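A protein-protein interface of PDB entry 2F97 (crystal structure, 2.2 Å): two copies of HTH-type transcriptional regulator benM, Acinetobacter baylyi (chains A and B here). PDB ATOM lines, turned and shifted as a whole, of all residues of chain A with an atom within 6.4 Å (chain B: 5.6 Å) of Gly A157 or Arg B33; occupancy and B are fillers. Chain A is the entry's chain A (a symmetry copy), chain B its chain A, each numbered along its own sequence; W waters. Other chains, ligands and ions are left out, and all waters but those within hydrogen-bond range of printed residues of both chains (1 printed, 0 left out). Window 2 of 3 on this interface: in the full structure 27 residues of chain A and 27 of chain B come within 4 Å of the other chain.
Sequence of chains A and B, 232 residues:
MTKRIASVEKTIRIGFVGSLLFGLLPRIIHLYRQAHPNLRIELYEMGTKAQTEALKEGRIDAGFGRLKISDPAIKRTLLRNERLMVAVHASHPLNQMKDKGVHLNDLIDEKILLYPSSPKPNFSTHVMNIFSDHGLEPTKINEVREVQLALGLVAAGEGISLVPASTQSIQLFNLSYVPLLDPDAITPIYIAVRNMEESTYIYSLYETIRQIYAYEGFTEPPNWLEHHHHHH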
ATOM      1  N   HIS A  89       1.619 -19.461  15.440  1.00  0.00           N
ATOM      2  CA  HIS A  89       1.213 -18.061  15.447  1.00  0.00           C
ATOM      3  C   HIS A  89       0.355 -17.825  16.689  1.00  0.00           C
ATOM      4  O   HIS A  89      -0.380 -18.717  17.111  1.00  0.00           O
ATOM      5  CB  HIS A  89       0.429 -17.706  14.183  1.00  0.00           C
ATOM      6  CG  HIS A  89       0.203 -16.235  14.009  1.00  0.00           C
ATOM      7  ND1 HIS A  89      -0.904 -15.588  14.516  1.00  0.00           N
ATOM      8  CD2 HIS A  89       0.947 -15.284  13.397  1.00  0.00           C
ATOM      9  CE1 HIS A  89      -0.836 -14.302  14.219  1.00  0.00           C
ATOM     10  NE2 HIS A  89       0.279 -14.091  13.540  1.00  0.00           N
ATOM     11  N   GLY A 152       9.875 -18.095  10.656  1.00  0.00           N
ATOM     12  CA  GLY A 152       9.395 -16.934   9.914  1.00  0.00           C
ATOM     13  C   GLY A 152       8.082 -17.180   9.192  1.00  0.00           C
ATOM     14  O   GLY A 152       7.208 -16.311   9.177  1.00  0.00           O
ATOM     15  N   LEU A 153       7.943 -18.366   8.600  1.00  0.00           N
ATOM     16  CA  LEU A 153       6.719 -18.752   7.900  1.00  0.00           C
ATOM     17  C   LEU A 153       5.556 -19.010   8.858  1.00  0.00           C
ATOM     18  O   LEU A 153       4.413 -18.677   8.545  1.00  0.00           O
ATOM     19  CB  LEU A 153       6.958 -19.968   6.994  1.00  0.00           C
ATOM     20  CG  LEU A 153       7.865 -19.769   5.768  1.00  0.00           C
ATOM     21  CD1 LEU A 153       8.255 -21.110   5.155  1.00  0.00           C
ATOM     22  CD2 LEU A 153       7.223 -18.867   4.726  1.00  0.00           C
ATOM     23  N   VAL A 154       5.850 -19.597  10.020  1.00  0.00           N
ATOM     24  CA  VAL A 154       4.859 -19.726  11.098  1.00  0.00           C
ATOM     25  C   VAL A 154       4.341 -18.345  11.517  1.00  0.00           C
ATOM     26  O   VAL A 154       3.130 -18.131  11.610  1.00  0.00           O
ATOM     27  CB  VAL A 154       5.428 -20.484  12.332  1.00  0.00           C
ATOM     28  CG1 VAL A 154       4.456 -20.419  13.501  1.00  0.00           C
ATOM     29  CG2 VAL A 154       5.723 -21.940  11.988  1.00  0.00           C
ATOM     30  N   ALA A 155       5.264 -17.410  11.743  1.00  0.00           N
ATOM     31  CA  ALA A 155       4.912 -16.030  12.082  1.00  0.00           C
ATOM     32  C   ALA A 155       4.135 -15.333  10.964  1.00  0.00           C
ATOM     33  O   ALA A 155       3.374 -14.397  11.223  1.00  0.00           O
ATOM     34  CB  ALA A 155       6.165 -15.232  12.445  1.00  0.00           C
ATOM     35  N   ALA A 156       4.330 -15.797   9.727  1.00  0.00           N
ATOM     36  CA  ALA A 156       3.625 -15.261   8.562  1.00  0.00           C
ATOM     37  C   ALA A 156       2.267 -15.936   8.319  1.00  0.00           C
ATOM     38  O   ALA A 156       1.505 -15.502   7.455  1.00  0.00           O
ATOM     39  CB  ALA A 156       4.504 -15.353   7.313  1.00  0.00           C
ATOM     40  N   GLY A 157       1.974 -16.986   9.084  1.00  0.00           N
ATOM     41  CA  GLY A 157       0.686 -17.680   9.007  1.00  0.00           C
ATOM     42  C   GLY A 157       0.651 -18.916   8.118  1.00  0.00           C
ATOM     43  O   GLY A 157      -0.425 -19.341   7.693  1.00  0.00           O
ATOM     44  N   GLU A 158       1.820 -19.499   7.850  1.00  0.00           N
ATOM     45  CA  GLU A 158       1.941 -20.625   6.911  1.00  0.00           C
ATOM     46  C   GLU A 158       1.708 -21.995   7.560  1.00  0.00           C
ATOM     47  O   GLU A 158       1.469 -22.986   6.864  1.00  0.00           O
ATOM     48  CB  GLU A 158       3.307 -20.598   6.215  1.00  0.00           C
ATOM     49  CG  GLU A 158       3.453 -21.549   5.026  1.00  0.00           C
ATOM     50  CD  GLU A 158       3.025 -20.923   3.713  1.00  0.00           C
ATOM     51  OE1 GLU A 158       3.631 -19.907   3.312  1.00  0.00           O
ATOM     52  OE2 GLU A 158       2.090 -21.455   3.073  1.00  0.00           O
ATOM     53  N   GLY A 159       1.780 -22.055   8.885  1.00  0.00           N
ATOM     54  CA  GLY A 159       1.519 -23.301   9.595  1.00  0.00           C
ATOM     55  C   GLY A 159       2.129 -23.340  10.978  1.00  0.00           C
ATOM     56  O   GLY A 159       2.180 -22.323  11.673  1.00  0.00           O
ATOM     57  N   PRO B  26       7.110 -10.903   8.261  1.00  0.00           N
ATOM     58  CA  PRO B  26       6.083 -11.905   8.573  1.00  0.00           C
ATOM     59  C   PRO B  26       4.731 -11.335   9.019  1.00  0.00           C
ATOM     60  O   PRO B  26       3.692 -11.842   8.595  1.00  0.00           O
ATOM     61  CB  PRO B  26       6.729 -12.740   9.684  1.00  0.00           C
ATOM     62  CG  PRO B  26       8.203 -12.596   9.437  1.00  0.00           C
ATOM     63  CD  PRO B  26       8.349 -11.152   9.025  1.00  0.00           C
ATOM     64  N   ILE B  28       3.548  -8.424   8.246  1.00  0.00           N
ATOM     65  CA  ILE B  28       2.984  -7.810   7.042  1.00  0.00           C
ATOM     66  C   ILE B  28       2.266  -8.881   6.211  1.00  0.00           C
ATOM     67  O   ILE B  28       1.122  -8.684   5.803  1.00  0.00           O
ATOM     68  CB  ILE B  28       4.057  -7.065   6.203  1.00  0.00           C
ATOM     69  CG1 ILE B  28       4.539  -5.811   6.944  1.00  0.00           C
ATOM     70  CG2 ILE B  28       3.503  -6.679   4.831  1.00  0.00           C
ATOM     71  CD1 ILE B  28       5.924  -5.319   6.520  1.00  0.00           C
ATOM     72  N   ILE B  29       2.932 -10.015   5.989  1.00  0.00           N
ATOM     73  CA  ILE B  29       2.332 -11.133   5.254  1.00  0.00           C
ATOM     74  C   ILE B  29       1.065 -11.636   5.949  1.00  0.00           C
ATOM     75  O   ILE B  29       0.055 -11.903   5.290  1.00  0.00           O
ATOM     76  CB  ILE B  29       3.324 -12.319   5.052  1.00  0.00           C
ATOM     77  CG1 ILE B  29       4.597 -11.875   4.310  1.00  0.00           C
ATOM     78  CG2 ILE B  29       2.643 -13.494   4.333  1.00  0.00           C
ATOM     79  CD1 ILE B  29       4.363 -11.216   2.948  1.00  0.00           C
ATOM     80  N   HIS B  30       1.121 -11.755   7.275  1.00  0.00           N
ATOM     81  CA  HIS B  30      -0.023 -12.246   8.037  1.00  0.00           C
ATOM     82  C   HIS B  30      -1.241 -11.326   7.917  1.00  0.00           C
ATOM     83  O   HIS B  30      -2.356 -11.804   7.727  1.00  0.00           O
ATOM     84  CB  HIS B  30       0.335 -12.491   9.504  1.00  0.00           C
ATOM     85  CG  HIS B  30      -0.687 -13.306  10.233  1.00  0.00           C
ATOM     86  ND1 HIS B  30      -1.818 -12.754  10.794  1.00  0.00           N
ATOM     87  CD2 HIS B  30      -0.762 -14.637  10.472  1.00  0.00           C
ATOM     88  CE1 HIS B  30      -2.540 -13.706  11.356  1.00  0.00           C
ATOM     89  NE2 HIS B  30      -1.922 -14.859  11.174  1.00  0.00           N
ATOM     90  N   LEU B  31      -1.023 -10.015   8.030  1.00  0.00           N
ATOM     91  CA  LEU B  31      -2.108  -9.039   7.894  1.00  0.00           C
ATOM     92  C   LEU B  31      -2.678  -9.041   6.473  1.00  0.00           C
ATOM     93  O   LEU B  31      -3.895  -9.024   6.287  1.00  0.00           O
ATOM     94  CB  LEU B  31      -1.648  -7.634   8.305  1.00  0.00           C
ATOM     95  CG  LEU B  31      -2.701  -6.514   8.377  1.00  0.00           C
ATOM     96  CD1 LEU B  31      -3.793  -6.815   9.407  1.00  0.00           C
ATOM     97  CD2 LEU B  31      -2.046  -5.172   8.675  1.00  0.00           C
ATOM     98  N   TYR B  32      -1.784  -9.075   5.486  1.00  0.00           N
ATOM     99  CA  TYR B  32      -2.147  -9.225   4.078  1.00  0.00           C
ATOM    100  C   TYR B  32      -3.006 -10.473   3.854  1.00  0.00           C
ATOM    101  O   TYR B  32      -3.990 -10.433   3.107  1.00  0.00           O
ATOM    102  CB  TYR B  32      -0.870  -9.286   3.233  1.00  0.00           C
ATOM    103  CG  TYR B  32      -1.069  -9.390   1.737  1.00  0.00           C
ATOM    104  CD1 TYR B  32      -1.676  -8.360   1.017  1.00  0.00           C
ATOM    105  CD2 TYR B  32      -0.613 -10.505   1.034  1.00  0.00           C
ATOM    106  CE1 TYR B  32      -1.845  -8.450  -0.360  1.00  0.00           C
ATOM    107  CE2 TYR B  32      -0.775 -10.603  -0.345  1.00  0.00           C
ATOM    108  CZ  TYR B  32      -1.390  -9.572  -1.034  1.00  0.00           C
ATOM    109  OH  TYR B  32      -1.554  -9.664  -2.398  1.00  0.00           O
ATOM    110  N   ARG B  33      -2.631 -11.563   4.524  1.00  0.00           N
ATOM    111  CA  ARG B  33      -3.337 -12.844   4.462  1.00  0.00           C
ATOM    112  C   ARG B  33      -4.782 -12.726   4.959  1.00  0.00           C
ATOM    113  O   ARG B  33      -5.689 -13.337   4.384  1.00  0.00           O
ATOM    114  CB  ARG B  33      -2.581 -13.902   5.282  1.00  0.00           C
ATOM    115  CG  ARG B  33      -2.495 -15.278   4.640  1.00  0.00           C
ATOM    116  CD  ARG B  33      -1.548 -16.207   5.415  1.00  0.00           C
ATOM    117  NE  ARG B  33      -0.947 -17.234   4.557  1.00  0.00           N
ATOM    118  CZ  ARG B  33       0.363 -17.388   4.362  1.00  0.00           C
ATOM    119  NH1 ARG B  33       1.234 -16.598   4.973  1.00  0.00           N
ATOM    120  NH2 ARG B  33       0.812 -18.349   3.562  1.00  0.00           N
ATOM    121  N   GLN B  34      -4.980 -11.942   6.018  1.00  0.00           N
ATOM    122  CA  GLN B  34      -6.306 -11.717   6.600  1.00  0.00           C
ATOM    123  C   GLN B  34      -7.211 -10.899   5.680  1.00  0.00           C
ATOM    124  O   GLN B  34      -8.426 -11.109   5.648  1.00  0.00           O
ATOM    125  CB  GLN B  34      -6.189 -11.026   7.964  1.00  0.00           C
ATOM    126  CG  GLN B  34      -5.597 -11.896   9.068  1.00  0.00           C
ATOM    127  CD  GLN B  34      -5.568 -11.201  10.422  1.00  0.00           C
ATOM    128  OE1 GLN B  34      -5.308  -9.999  10.516  1.00  0.00           O
ATOM    129  NE2 GLN B  34      -5.829 -11.961  11.478  1.00  0.00           N
ATOM    130  N   ALA B  35      -6.612  -9.971   4.936  1.00  0.00           N
ATOM    131  CA  ALA B  35      -7.346  -9.101   4.007  1.00  0.00           C
ATOM    132  C   ALA B  35      -7.838  -9.844   2.765  1.00  0.00           C
ATOM    133  O   ALA B  35      -8.796  -9.415   2.120  1.00  0.00           O
ATOM    134  CB  ALA B  35      -6.490  -7.907   3.608  1.00  0.00           C
ATOM    135  N   HIS B  36      -7.174 -10.951   2.433  1.00  0.00           N
ATOM    136  CA  HIS B  36      -7.560 -11.781   1.295  1.00  0.00           C
ATOM    137  C   HIS B  36      -7.650 -13.258   1.698  1.00  0.00           C
ATOM    138  O   HIS B  36      -6.730 -14.031   1.426  1.00  0.00           O
ATOM    139  CB  HIS B  36      -6.571 -11.607   0.136  1.00  0.00           C
ATOM    140  CG  HIS B  36      -6.266 -10.179  -0.196  1.00  0.00           C
ATOM    141  ND1 HIS B  36      -7.069  -9.417  -1.018  1.00  0.00           N
ATOM    142  CD2 HIS B  36      -5.244  -9.377   0.182  1.00  0.00           C
ATOM    143  CE1 HIS B  36      -6.554  -8.205  -1.129  1.00  0.00           C
ATOM    144  NE2 HIS B  36      -5.446  -8.156  -0.412  1.00  0.00           N
ATOM    145  N   PRO B  37      -8.764 -13.658   2.347  1.00  0.00           N
ATOM    146  CA  PRO B  37      -8.933 -15.041   2.813  1.00  0.00           C
ATOM    147  C   PRO B  37      -8.965 -16.092   1.695  1.00  0.00           C
ATOM    148  O   PRO B  37      -8.572 -17.236   1.924  1.00  0.00           O
ATOM    149  CB  PRO B  37     -10.280 -15.005   3.547  1.00  0.00           C
ATOM    150  CG  PRO B  37     -10.997 -13.831   2.982  1.00  0.00           C
ATOM    151  CD  PRO B  37      -9.933 -12.823   2.683  1.00  0.00           C
ATOM    152  N   ILE B  41      -1.302 -17.512  -1.199  1.00  0.00           N
ATOM    153  CA  ILE B  41      -0.038 -16.793  -1.101  1.00  0.00           C
ATOM    154  C   ILE B  41       1.117 -17.786  -1.062  1.00  0.00           C
ATOM    155  O   ILE B  41       1.166 -18.665  -0.197  1.00  0.00           O
ATOM    156  CB  ILE B  41       0.004 -15.864   0.139  1.00  0.00           C
ATOM    157  CG1 ILE B  41      -1.093 -14.799   0.046  1.00  0.00           C
ATOM    158  CG2 ILE B  41       1.381 -15.205   0.277  1.00  0.00           C
ATOM    159  CD1 ILE B  41      -1.419 -14.129   1.361  1.00  0.00           C
ATOM    160  N   LEU B  43       5.231 -18.145  -0.779  1.00  0.00           N
ATOM    161  CA  LEU B  43       6.414 -17.441  -0.304  1.00  0.00           C
ATOM    162  C   LEU B  43       7.678 -18.196  -0.699  1.00  0.00           C
ATOM    163  O   LEU B  43       7.790 -19.398  -0.452  1.00  0.00           O
ATOM    164  CB  LEU B  43       6.341 -17.248   1.215  1.00  0.00           C
ATOM    165  CG  LEU B  43       5.089 -16.518   1.728  1.00  0.00           C
ATOM    166  CD1 LEU B  43       4.952 -16.646   3.239  1.00  0.00           C
ATOM    167  CD2 LEU B  43       5.081 -15.046   1.308  1.00  0.00           C
HETATM  168  O   HOH W   1       4.439 -20.536   0.643  1.00  0.00           O
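Of the 9 printed residues of chain A, 7 touch a printed residue of chain B.
Of the 13 printed residues of chain B, 5 touch a printed residue of chain A.
Hydrophobic or aromatic side chains of chain B that line the printed part of chain A: Pro B26, Ile B29, His B30 and Leu B43.
Among the printed residues, 13 pairs touch across the chains.
Among the printed residues, Asp or Glu carboxylates within 4 Å of a Lys or Arg side-chain nitrogen of the other chain: Glu A158 with Arg B33 (3.2 Å).
Gly A157 touches just these residues of chain B: His B30 (3.7 Å) and Arg B33 (3.8 Å).
Arg B33 touches three residues of chain A.
Printed residues of chain B within 4 Å of Ala A155: Pro B26 (3.7 Å) and His B30 (3.98 Å).
Of the printed residues of chain B, Gly A152 touches Pro B26 (3.6 Å).
Of the printed residues of chain B, Leu A153 touches Leu B43 (3.5 Å).
Of the printed residues of chain B, Glu A158 touches Arg B33 (3.2 Å) and Leu B43 (3.5 Å).
Of the printed residues of chain A, His B30 touches His A89, Ala A155, Ala A156 and Gly A157.
Ile B41 touches none of the printed residues of chain A.
The nearest residue of chain A that does not touch Arg B33 is Leu A153 (5.2 Å).
A ring nitrogen (NE2) of His B30 sits close to a ring nitrogen (NE2) of His A89, at 3.3 Å.
The backbone carbonyl oxygen (O) of Ala A156 lies within hydrogen-bond range of the guanidinium group (NH1) of Arg B33, at 2.7 Å.
The side-chain carboxylate of Glu A158 is in salt-bridge range of the guanidinium group of Arg B33 (3.2 Å).
No position is printed for both chains.
Water W1 lies within hydrogen-bond range of OE1 of Glu A158 (2.9 Å) and N of Leu B43 (2.9 Å).
Gly A152 touches Pro B26.
Leu A153 touches Leu B43 (CD2 to CD1, 3.5 Å).
Ala A155 touches Pro B26.
O of Ala A155 touches CB of His B30 (3.98 Å).
O of Pro B26 touches CA of Ala A156 (3.4 Å).
Ala A156 touches Ile B29 (O to CG2, 3.9 Å).
Ala A156 touches His B30.
Gly A157 touches His B30 (CA to CD2, 3.7 Å).
NE of Arg B33 touches O of Gly A157, 3.8 Å away.
CD1 of Leu B43 touches OE1 of Glu A158, 3.5 Å away.
The backbone carbonyl oxygen of Leu A153 is in hydrogen-bond range of the backbone NH of Glu A158, 2.8 Å away.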
